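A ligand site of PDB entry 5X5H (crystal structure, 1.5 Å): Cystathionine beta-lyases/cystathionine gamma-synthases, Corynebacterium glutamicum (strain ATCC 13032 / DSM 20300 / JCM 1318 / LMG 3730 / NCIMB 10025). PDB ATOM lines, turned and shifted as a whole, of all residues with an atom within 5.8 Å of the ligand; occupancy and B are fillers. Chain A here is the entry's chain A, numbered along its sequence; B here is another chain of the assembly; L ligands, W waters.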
ATOM      1  N   SER A  81      -7.818 -32.982 -17.424  1.00  0.00           N
ATOM      2  CA  SER A  81      -8.914 -32.042 -17.118  1.00  0.00           C
ATOM      3  C   SER A  81      -9.033 -32.029 -15.619  1.00  0.00           C
ATOM      4  O   SER A  81      -8.565 -32.903 -14.891  1.00  0.00           O
ATOM      5  CB  SER A  81     -10.224 -32.408 -17.833  1.00  0.00           C
ATOM      6  OG  SER A  81     -10.697 -33.661 -17.255  1.00  0.00           O
ATOM      7  N   GLY A  82      -9.723 -31.008 -15.130  1.00  0.00           N
ATOM      8  CA  GLY A  82     -10.157 -30.951 -13.713  1.00  0.00           C
ATOM      9  C   GLY A  82     -10.991 -32.158 -13.333  1.00  0.00           C
ATOM     10  O   GLY A  82     -10.768 -32.790 -12.251  1.00  0.00           O
ATOM     11  N   MET A  83     -11.933 -32.537 -14.184  1.00  0.00           N
ATOM     12  CA  MET A  83     -12.688 -33.729 -13.940  1.00  0.00           C
ATOM     13  C   MET A  83     -11.904 -34.961 -13.858  1.00  0.00           C
ATOM     14  O   MET A  83     -12.130 -35.844 -13.020  1.00  0.00           O
ATOM     15  CB  MET A  83     -13.775 -33.907 -14.988  1.00  0.00           C
ATOM     16  CG  MET A  83     -14.946 -32.932 -14.866  1.00  0.00           C
ATOM     17  SD  MET A  83     -15.736 -32.811 -13.234  1.00  0.00           S
ATOM     18  CE  MET A  83     -15.807 -34.519 -12.767  1.00  0.00           C
ATOM     19  N   ALA A  84     -10.900 -35.135 -14.715  1.00  0.00           N
ATOM     20  CA  ALA A  84     -10.113 -36.389 -14.653  1.00  0.00           C
ATOM     21  C   ALA A  84      -9.272 -36.431 -13.433  1.00  0.00           C
ATOM     22  O   ALA A  84      -9.048 -37.499 -12.815  1.00  0.00           O
ATOM     23  CB  ALA A  84      -9.162 -36.483 -15.858  1.00  0.00           C
ATOM     24  N   THR A  86     -10.157 -35.090 -10.587  1.00  0.00           N
ATOM     25  CA  THR A  86     -11.145 -35.406  -9.505  1.00  0.00           C
ATOM     26  C   THR A  86     -11.366 -36.921  -9.525  1.00  0.00           C
ATOM     27  O   THR A  86     -11.353 -37.555  -8.460  1.00  0.00           O
ATOM     28  CB  THR A  86     -12.447 -34.643  -9.768  1.00  0.00           C
ATOM     29  OG1 THR A  86     -12.195 -33.212  -9.696  1.00  0.00           O
ATOM     30  CG2 THR A  86     -13.529 -34.969  -8.736  1.00  0.00           C
ATOM     31  N   TYR A 107     -19.670 -27.672  -8.312  1.00  0.00           N
ATOM     32  CA  TYR A 107     -19.642 -27.813  -9.671  1.00  0.00           C
ATOM     33  C   TYR A 107     -20.500 -29.093  -9.988  1.00  0.00           C
ATOM     34  O   TYR A 107     -20.351 -30.205  -9.407  1.00  0.00           O
ATOM     35  CB  TYR A 107     -18.145 -27.905 -10.213  1.00  0.00           C
ATOM     36  CG  TYR A 107     -18.122 -28.131 -11.614  1.00  0.00           C
ATOM     37  CD1 TYR A 107     -18.781 -27.270 -12.552  1.00  0.00           C
ATOM     38  CD2 TYR A 107     -17.473 -29.217 -12.202  1.00  0.00           C
ATOM     39  CE1 TYR A 107     -18.845 -27.488 -13.931  1.00  0.00           C
ATOM     40  CE2 TYR A 107     -17.504 -29.410 -13.514  1.00  0.00           C
ATOM     41  CZ  TYR A 107     -18.142 -28.584 -14.470  1.00  0.00           C
ATOM     42  OH  TYR A 107     -18.245 -28.865 -15.831  1.00  0.00           O
ATOM     43  N   THR A 110     -18.702 -32.419 -10.647  1.00  0.00           N
ATOM     44  CA  THR A 110     -18.291 -33.121  -9.476  1.00  0.00           C
ATOM     45  C   THR A 110     -19.454 -34.005  -8.903  1.00  0.00           C
ATOM     46  O   THR A 110     -19.316 -35.191  -8.586  1.00  0.00           O
ATOM     47  CB  THR A 110     -17.717 -32.229  -8.379  1.00  0.00           C
ATOM     48  OG1 THR A 110     -16.696 -31.400  -8.973  1.00  0.00           O
ATOM     49  CG2 THR A 110     -17.199 -33.022  -7.270  1.00  0.00           C
ATOM     50  N   GLU A 150     -15.464 -27.127  -1.894  1.00  0.00           N
ATOM     51  CA  GLU A 150     -15.131 -26.077  -2.836  1.00  0.00           C
ATOM     52  C   GLU A 150     -15.309 -24.800  -2.114  1.00  0.00           C
ATOM     53  O   GLU A 150     -16.380 -24.582  -1.524  1.00  0.00           O
ATOM     54  CB  GLU A 150     -16.078 -25.959  -3.977  1.00  0.00           C
ATOM     55  CG  GLU A 150     -15.963 -26.869  -5.020  1.00  0.00           C
ATOM     56  CD  GLU A 150     -16.985 -26.645  -6.109  1.00  0.00           C
ATOM     57  OE1 GLU A 150     -17.517 -25.545  -6.394  1.00  0.00           O
ATOM     58  OE2 GLU A 150     -17.220 -27.623  -6.791  1.00  0.00           O
ATOM     59  N   ASN A 154     -19.053 -23.002  -6.745  1.00  0.00           N
ATOM     60  CA  ASN A 154     -19.475 -22.642  -8.081  1.00  0.00           C
ATOM     61  C   ASN A 154     -20.908 -23.083  -8.168  1.00  0.00           C
ATOM     62  O   ASN A 154     -21.127 -24.332  -8.076  1.00  0.00           O
ATOM     63  CB  ASN A 154     -18.642 -23.557  -9.050  1.00  0.00           C
ATOM     64  CG  ASN A 154     -18.960 -23.353 -10.482  1.00  0.00           C
ATOM     65  OD1 ASN A 154     -19.881 -22.607 -10.860  1.00  0.00           O
ATOM     66  ND2 ASN A 154     -18.094 -23.950 -11.376  1.00  0.00           N
ATOM     67  N   ASP A 179     -11.184 -28.160  -3.515  1.00  0.00           N
ATOM     68  CA  ASP A 179     -11.157 -27.727  -4.935  1.00  0.00           C
ATOM     69  C   ASP A 179     -10.952 -26.216  -4.883  1.00  0.00           C
ATOM     70  O   ASP A 179     -11.861 -25.469  -4.486  1.00  0.00           O
ATOM     71  CB  ASP A 179     -12.389 -28.174  -5.623  1.00  0.00           C
ATOM     72  CG  ASP A 179     -12.506 -27.686  -7.066  1.00  0.00           C
ATOM     73  OD1 ASP A 179     -11.771 -26.745  -7.470  1.00  0.00           O
ATOM     74  OD2 ASP A 179     -13.442 -28.226  -7.785  1.00  0.00           O
ATOM     75  N   THR A 181     -10.076 -24.155  -7.378  1.00  0.00           N
ATOM     76  CA  THR A 181     -10.130 -23.608  -8.726  1.00  0.00           C
ATOM     77  C   THR A 181     -10.434 -22.121  -8.699  1.00  0.00           C
ATOM     78  O   THR A 181      -9.754 -21.344  -9.379  1.00  0.00           O
ATOM     79  CB  THR A 181     -11.120 -24.369  -9.585  1.00  0.00           C
ATOM     80  OG1 THR A 181     -10.725 -25.765  -9.726  1.00  0.00           O
ATOM     81  CG2 THR A 181     -11.320 -23.797 -10.923  1.00  0.00           C
ATOM     82  N   PHE A 182     -11.551 -21.724  -8.073  1.00  0.00           N
ATOM     83  CA  PHE A 182     -12.011 -20.309  -8.125  1.00  0.00           C
ATOM     84  C   PHE A 182     -11.078 -19.357  -7.439  1.00  0.00           C
ATOM     85  O   PHE A 182     -10.774 -18.278  -8.032  1.00  0.00           O
ATOM     86  CB  PHE A 182     -13.387 -20.217  -7.475  1.00  0.00           C
ATOM     87  CG  PHE A 182     -14.489 -20.470  -8.369  1.00  0.00           C
ATOM     88  CD1 PHE A 182     -14.489 -21.438  -9.397  1.00  0.00           C
ATOM     89  CD2 PHE A 182     -15.728 -19.819  -8.128  1.00  0.00           C
ATOM     90  CE1 PHE A 182     -15.588 -21.599 -10.242  1.00  0.00           C
ATOM     91  CE2 PHE A 182     -16.806 -20.009  -8.939  1.00  0.00           C
ATOM     92  CZ  PHE A 182     -16.773 -20.875  -9.998  1.00  0.00           C
ATOM     93  N   LEU A 199      -7.154 -29.662  -5.305  1.00  0.00           N
ATOM     94  CA  LEU A 199      -7.473 -29.884  -6.705  1.00  0.00           C
ATOM     95  C   LEU A 199      -7.640 -28.564  -7.411  1.00  0.00           C
ATOM     96  O   LEU A 199      -8.342 -27.680  -6.909  1.00  0.00           O
ATOM     97  CB  LEU A 199      -8.727 -30.710  -6.775  1.00  0.00           C
ATOM     98  CG  LEU A 199      -9.461 -31.185  -8.054  1.00  0.00           C
ATOM     99  CD1 LEU A 199     -10.077 -30.079  -8.836  1.00  0.00           C
ATOM    100  CD2 LEU A 199      -8.703 -32.009  -8.955  1.00  0.00           C
ATOM    101  N   SER A 201      -8.926 -27.235 -11.486  1.00  0.00           N
ATOM    102  CA  SER A 201      -9.151 -27.194 -12.949  1.00  0.00           C
ATOM    103  C   SER A 201      -8.210 -26.082 -13.492  1.00  0.00           C
ATOM    104  O   SER A 201      -8.517 -24.932 -13.276  1.00  0.00           O
ATOM    105  CB  SER A 201     -10.542 -26.881 -13.271  1.00  0.00           C
ATOM    106  OG  SER A 201     -10.613 -26.604 -14.699  1.00  0.00           O
ATOM    107  N   THR A 202      -7.093 -26.421 -14.107  1.00  0.00           N
ATOM    108  CA  THR A 202      -6.207 -25.419 -14.673  1.00  0.00           C
ATOM    109  C   THR A 202      -6.777 -24.826 -15.915  1.00  0.00           C
ATOM    110  O   THR A 202      -6.276 -23.795 -16.423  1.00  0.00           O
ATOM    111  CB  THR A 202      -4.821 -26.000 -14.892  1.00  0.00           C
ATOM    112  OG1 THR A 202      -4.873 -27.073 -15.873  1.00  0.00           O
ATOM    113  CG2 THR A 202      -4.206 -26.576 -13.663  1.00  0.00           C
ATOM    114  N   THR A 203      -7.875 -25.410 -16.462  1.00  0.00           N
ATOM    115  CA  THR A 203      -8.677 -24.820 -17.528  1.00  0.00           C
ATOM    116  C   THR A 203      -9.039 -23.385 -17.290  1.00  0.00           C
ATOM    117  O   THR A 203      -9.289 -22.641 -18.244  1.00  0.00           O
ATOM    118  CB  THR A 203      -9.949 -25.684 -17.635  1.00  0.00           C
ATOM    119  OG1 THR A 203      -9.568 -27.057 -17.730  1.00  0.00           O
ATOM    120  CG2 THR A 203     -10.725 -25.314 -18.889  1.00  0.00           C
ATOM    121  N   LYS A 204      -9.209 -23.056 -16.024  1.00  0.00           N
ATOM    122  CA  LYS A 204      -9.738 -21.768 -15.593  1.00  0.00           C
ATOM    123  C   LYS A 204      -8.605 -20.756 -15.342  1.00  0.00           C
ATOM    124  O   LYS A 204      -7.945 -20.423 -16.300  1.00  0.00           O
ATOM    125  CB  LYS A 204     -10.682 -21.997 -14.405  1.00  0.00           C
ATOM    126  CG  LYS A 204     -11.699 -23.078 -14.458  1.00  0.00           C
ATOM    127  CD  LYS A 204     -12.437 -23.115 -15.680  1.00  0.00           C
ATOM    128  CE  LYS A 204     -13.570 -24.282 -15.732  1.00  0.00           C
ATOM    129  NZ  LYS A 204     -14.337 -24.852 -14.547  1.00  0.00           N
ATOM    130  N   VAL A 213      -7.577 -27.257 -21.646  1.00  0.00           N
ATOM    131  CA  VAL A 213      -8.292 -28.010 -20.611  1.00  0.00           C
ATOM    132  C   VAL A 213      -7.208 -28.744 -19.819  1.00  0.00           C
ATOM    133  O   VAL A 213      -6.333 -29.371 -20.411  1.00  0.00           O
ATOM    134  CB  VAL A 213      -9.301 -28.938 -21.216  1.00  0.00           C
ATOM    135  CG1 VAL A 213      -9.961 -29.766 -20.150  1.00  0.00           C
ATOM    136  CG2 VAL A 213     -10.352 -28.162 -22.004  1.00  0.00           C
ATOM    137  N   GLY A 214      -7.274 -28.730 -18.506  1.00  0.00           N
ATOM    138  CA  GLY A 214      -6.305 -29.428 -17.667  1.00  0.00           C
ATOM    139  C   GLY A 214      -6.719 -29.466 -16.203  1.00  0.00           C
ATOM    140  O   GLY A 214      -7.565 -28.686 -15.773  1.00  0.00           O
ATOM    141  N   GLY A 215      -6.149 -30.427 -15.454  1.00  0.00           N
ATOM    142  CA  GLY A 215      -6.307 -30.519 -14.010  1.00  0.00           C
ATOM    143  C   GLY A 215      -5.041 -30.763 -13.307  1.00  0.00           C
ATOM    144  O   GLY A 215      -4.018 -31.127 -13.954  1.00  0.00           O
ATOM    145  N   LEU A 333     -14.839 -20.083 -17.264  1.00  0.00           N
ATOM    146  CA  LEU A 333     -14.458 -18.976 -16.403  1.00  0.00           C
ATOM    147  C   LEU A 333     -12.979 -18.880 -16.260  1.00  0.00           C
ATOM    148  O   LEU A 333     -12.239 -19.838 -16.646  1.00  0.00           O
ATOM    149  CB  LEU A 333     -15.171 -19.122 -15.002  1.00  0.00           C
ATOM    150  CG  LEU A 333     -14.721 -20.323 -14.217  1.00  0.00           C
ATOM    151  CD1 LEU A 333     -13.768 -20.002 -13.109  1.00  0.00           C
ATOM    152  CD2 LEU A 333     -15.878 -21.169 -13.730  1.00  0.00           C
ATOM    153  N   ARG A 364     -24.115 -16.169 -13.485  1.00  0.00           N
ATOM    154  CA  ARG A 364     -22.753 -16.254 -12.984  1.00  0.00           C
ATOM    155  C   ARG A 364     -21.880 -15.509 -13.971  1.00  0.00           C
ATOM    156  O   ARG A 364     -21.965 -15.698 -15.191  1.00  0.00           O
ATOM    157  CB  ARG A 364     -22.286 -17.666 -12.874  1.00  0.00           C
ATOM    158  CG  ARG A 364     -20.899 -17.872 -12.283  1.00  0.00           C
ATOM    159  CD  ARG A 364     -20.353 -19.279 -12.434  1.00  0.00           C
ATOM    160  NE  ARG A 364     -19.862 -19.442 -13.771  1.00  0.00           N
ATOM    161  CZ  ARG A 364     -19.574 -20.611 -14.296  1.00  0.00           C
ATOM    162  NH1 ARG A 364     -19.601 -21.688 -13.587  1.00  0.00           N
ATOM    163  NH2 ARG A 364     -19.112 -20.692 -15.473  1.00  0.00           N
ATOM    164  N   TYR B  52     -18.264 -26.612 -24.847  1.00  0.00           N
ATOM    165  CA  TYR B  52     -17.180 -26.621 -23.879  1.00  0.00           C
ATOM    166  C   TYR B  52     -16.311 -27.780 -24.324  1.00  0.00           C
ATOM    167  O   TYR B  52     -16.825 -28.884 -24.585  1.00  0.00           O
ATOM    168  CB  TYR B  52     -17.719 -26.851 -22.464  1.00  0.00           C
ATOM    169  CG  TYR B  52     -16.666 -26.760 -21.416  1.00  0.00           C
ATOM    170  CD1 TYR B  52     -16.075 -25.527 -21.046  1.00  0.00           C
ATOM    171  CD2 TYR B  52     -16.294 -27.850 -20.691  1.00  0.00           C
ATOM    172  CE1 TYR B  52     -15.081 -25.498 -20.058  1.00  0.00           C
ATOM    173  CE2 TYR B  52     -15.310 -27.824 -19.731  1.00  0.00           C
ATOM    174  CZ  TYR B  52     -14.756 -26.624 -19.374  1.00  0.00           C
ATOM    175  OH  TYR B  52     -13.843 -26.502 -18.353  1.00  0.00           O
ATOM    176  N   ARG B  54     -14.241 -30.033 -23.135  1.00  0.00           N
ATOM    177  CA  ARG B  54     -14.322 -31.356 -22.509  1.00  0.00           C
ATOM    178  C   ARG B  54     -15.550 -32.130 -22.945  1.00  0.00           C
ATOM    179  O   ARG B  54     -15.524 -33.369 -23.077  1.00  0.00           O
ATOM    180  CB  ARG B  54     -14.351 -31.171 -20.975  1.00  0.00           C
ATOM    181  CG  ARG B  54     -14.574 -32.539 -20.293  1.00  0.00           C
ATOM    182  CD  ARG B  54     -14.335 -32.606 -18.828  1.00  0.00           C
ATOM    183  NE  ARG B  54     -14.643 -31.501 -18.058  1.00  0.00           N
ATOM    184  CZ  ARG B  54     -15.857 -31.082 -17.695  1.00  0.00           C
ATOM    185  NH1 ARG B  54     -15.972 -30.011 -16.991  1.00  0.00           N
ATOM    186  NH2 ARG B  54     -16.946 -31.697 -18.088  1.00  0.00           N
HETATM  187  N1  LIG L   1     -14.144 -27.617 -10.314  1.00  0.00           N
HETATM  188  C1  LIG L   1     -14.613 -26.405 -10.518  1.00  0.00           C
HETATM  189  C2  LIG L   1     -14.794 -25.543  -9.315  1.00  0.00           C
HETATM  190  C3  LIG L   1     -14.725 -25.919 -11.779  1.00  0.00           C
HETATM  191  O1  LIG L   1     -15.170 -24.646 -12.046  1.00  0.00           O
HETATM  192  C4  LIG L   1     -14.451 -26.722 -12.899  1.00  0.00           C
HETATM  193  C5  LIG L   1     -14.616 -26.181 -14.258  1.00  0.00           C
HETATM  194  C6  LIG L   1     -14.124 -28.079 -12.677  1.00  0.00           C
HETATM  195  C7  LIG L   1     -13.965 -28.463 -11.357  1.00  0.00           C
HETATM  196  C8  LIG L   1     -13.915 -29.099 -13.794  1.00  0.00           C
HETATM  197  O2  LIG L   1     -12.667 -28.860 -14.527  1.00  0.00           O
HETATM  198  P1  LIG L   1     -12.560 -29.220 -16.067  1.00  0.00           P
HETATM  199  O3  LIG L   1     -13.638 -28.446 -16.797  1.00  0.00           O
HETATM  200  O4  LIG L   1     -11.136 -28.770 -16.318  1.00  0.00           O
HETATM  201  O5  LIG L   1     -12.715 -30.740 -16.205  1.00  0.00           O
HETATM  202  O   HOH W   1     -15.713 -23.432  -6.970  1.00  0.00           O
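NZ of Lys 204 is covalently linked to C5 of the ligand (1.4 Å). OH of Tyr 52 of chain B lies within hydrogen-bond range of O3 of the ligand (2.5 Å). OD2 of Asp 179 lies within hydrogen-bond range of N1 of the ligand (2.7 Å). OG1 of Thr 203 is in hydrogen-bond range of O4 of the ligand (2.7 Å). An oxygen (O4) of the ligand sits at hydrogen-bond distance from the side-chain hydroxyl (OG) of Ser 201, 2.8 Å away. NE of Arg 54 of chain B is in salt-bridge range of O5 of the ligand, 2.8 Å away. The backbone NH of Met 83 lies within hydrogen-bond range of an oxygen (O5) of the ligand (2.8 Å). An oxygen (O4) of the ligand sits at hydrogen-bond distance from the backbone NH (N) of Gly 82 (2.9 Å). ND2 of Asn 154 is in hydrogen-bond range of O1 of the ligand.
The side-chain hydroxyl (OG1) of Thr 181 lies within hydrogen-bond range of the side-chain carboxylate (OD1) of Asp 179. The side-chain hydroxyl (OG) of Ser 201 sits close to the side-chain hydroxyl (OG1) of Thr 203, at 3.2 Å. N of Gly 214 lies within hydrogen-bond range of OG1 of Thr 203, 2.9 Å away. OH of Tyr 107 is in hydrogen-bond range of NH1 of Arg 54 of chain B (2.8 Å). The backbone NH (N) of Met 83 sits close to the side-chain hydroxyl (OG) of Ser 81 (3.5 Å). The backbone NH (N) of Gly 82 lies within hydrogen-bond range of the backbone carbonyl oxygen (O) of Gly 214, at 3.2 Å. The backbone NH (N) of Asn 154 lies within hydrogen-bond range of the side-chain carboxylate (OE1) of Glu 150, 3.0 Å away. The backbone NH of Tyr 107 sits at hydrogen-bond distance from the side-chain carboxylate of Glu 150, 2.9 Å away.
Residues that only touch the ligand: Ser 81, Phe 182, Tyr 107, Gly 214, Thr 181, Leu 333 and Glu 150. Hydrophobic or aromatic side chains that line the ligand: Met 83, Tyr 107, Phe 182, Leu 333 and Tyr 52 of chain B. Of the 24 residues printed, 16 come within 4 Å of the ligand. The nearest printed residue that does not touch the ligand is Val 213 (4.1 Å).
Water W1 lies within hydrogen-bond range of the side-chain carboxylate (OE1) of Glu 150 and the backbone NH (N) of Asn 154.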
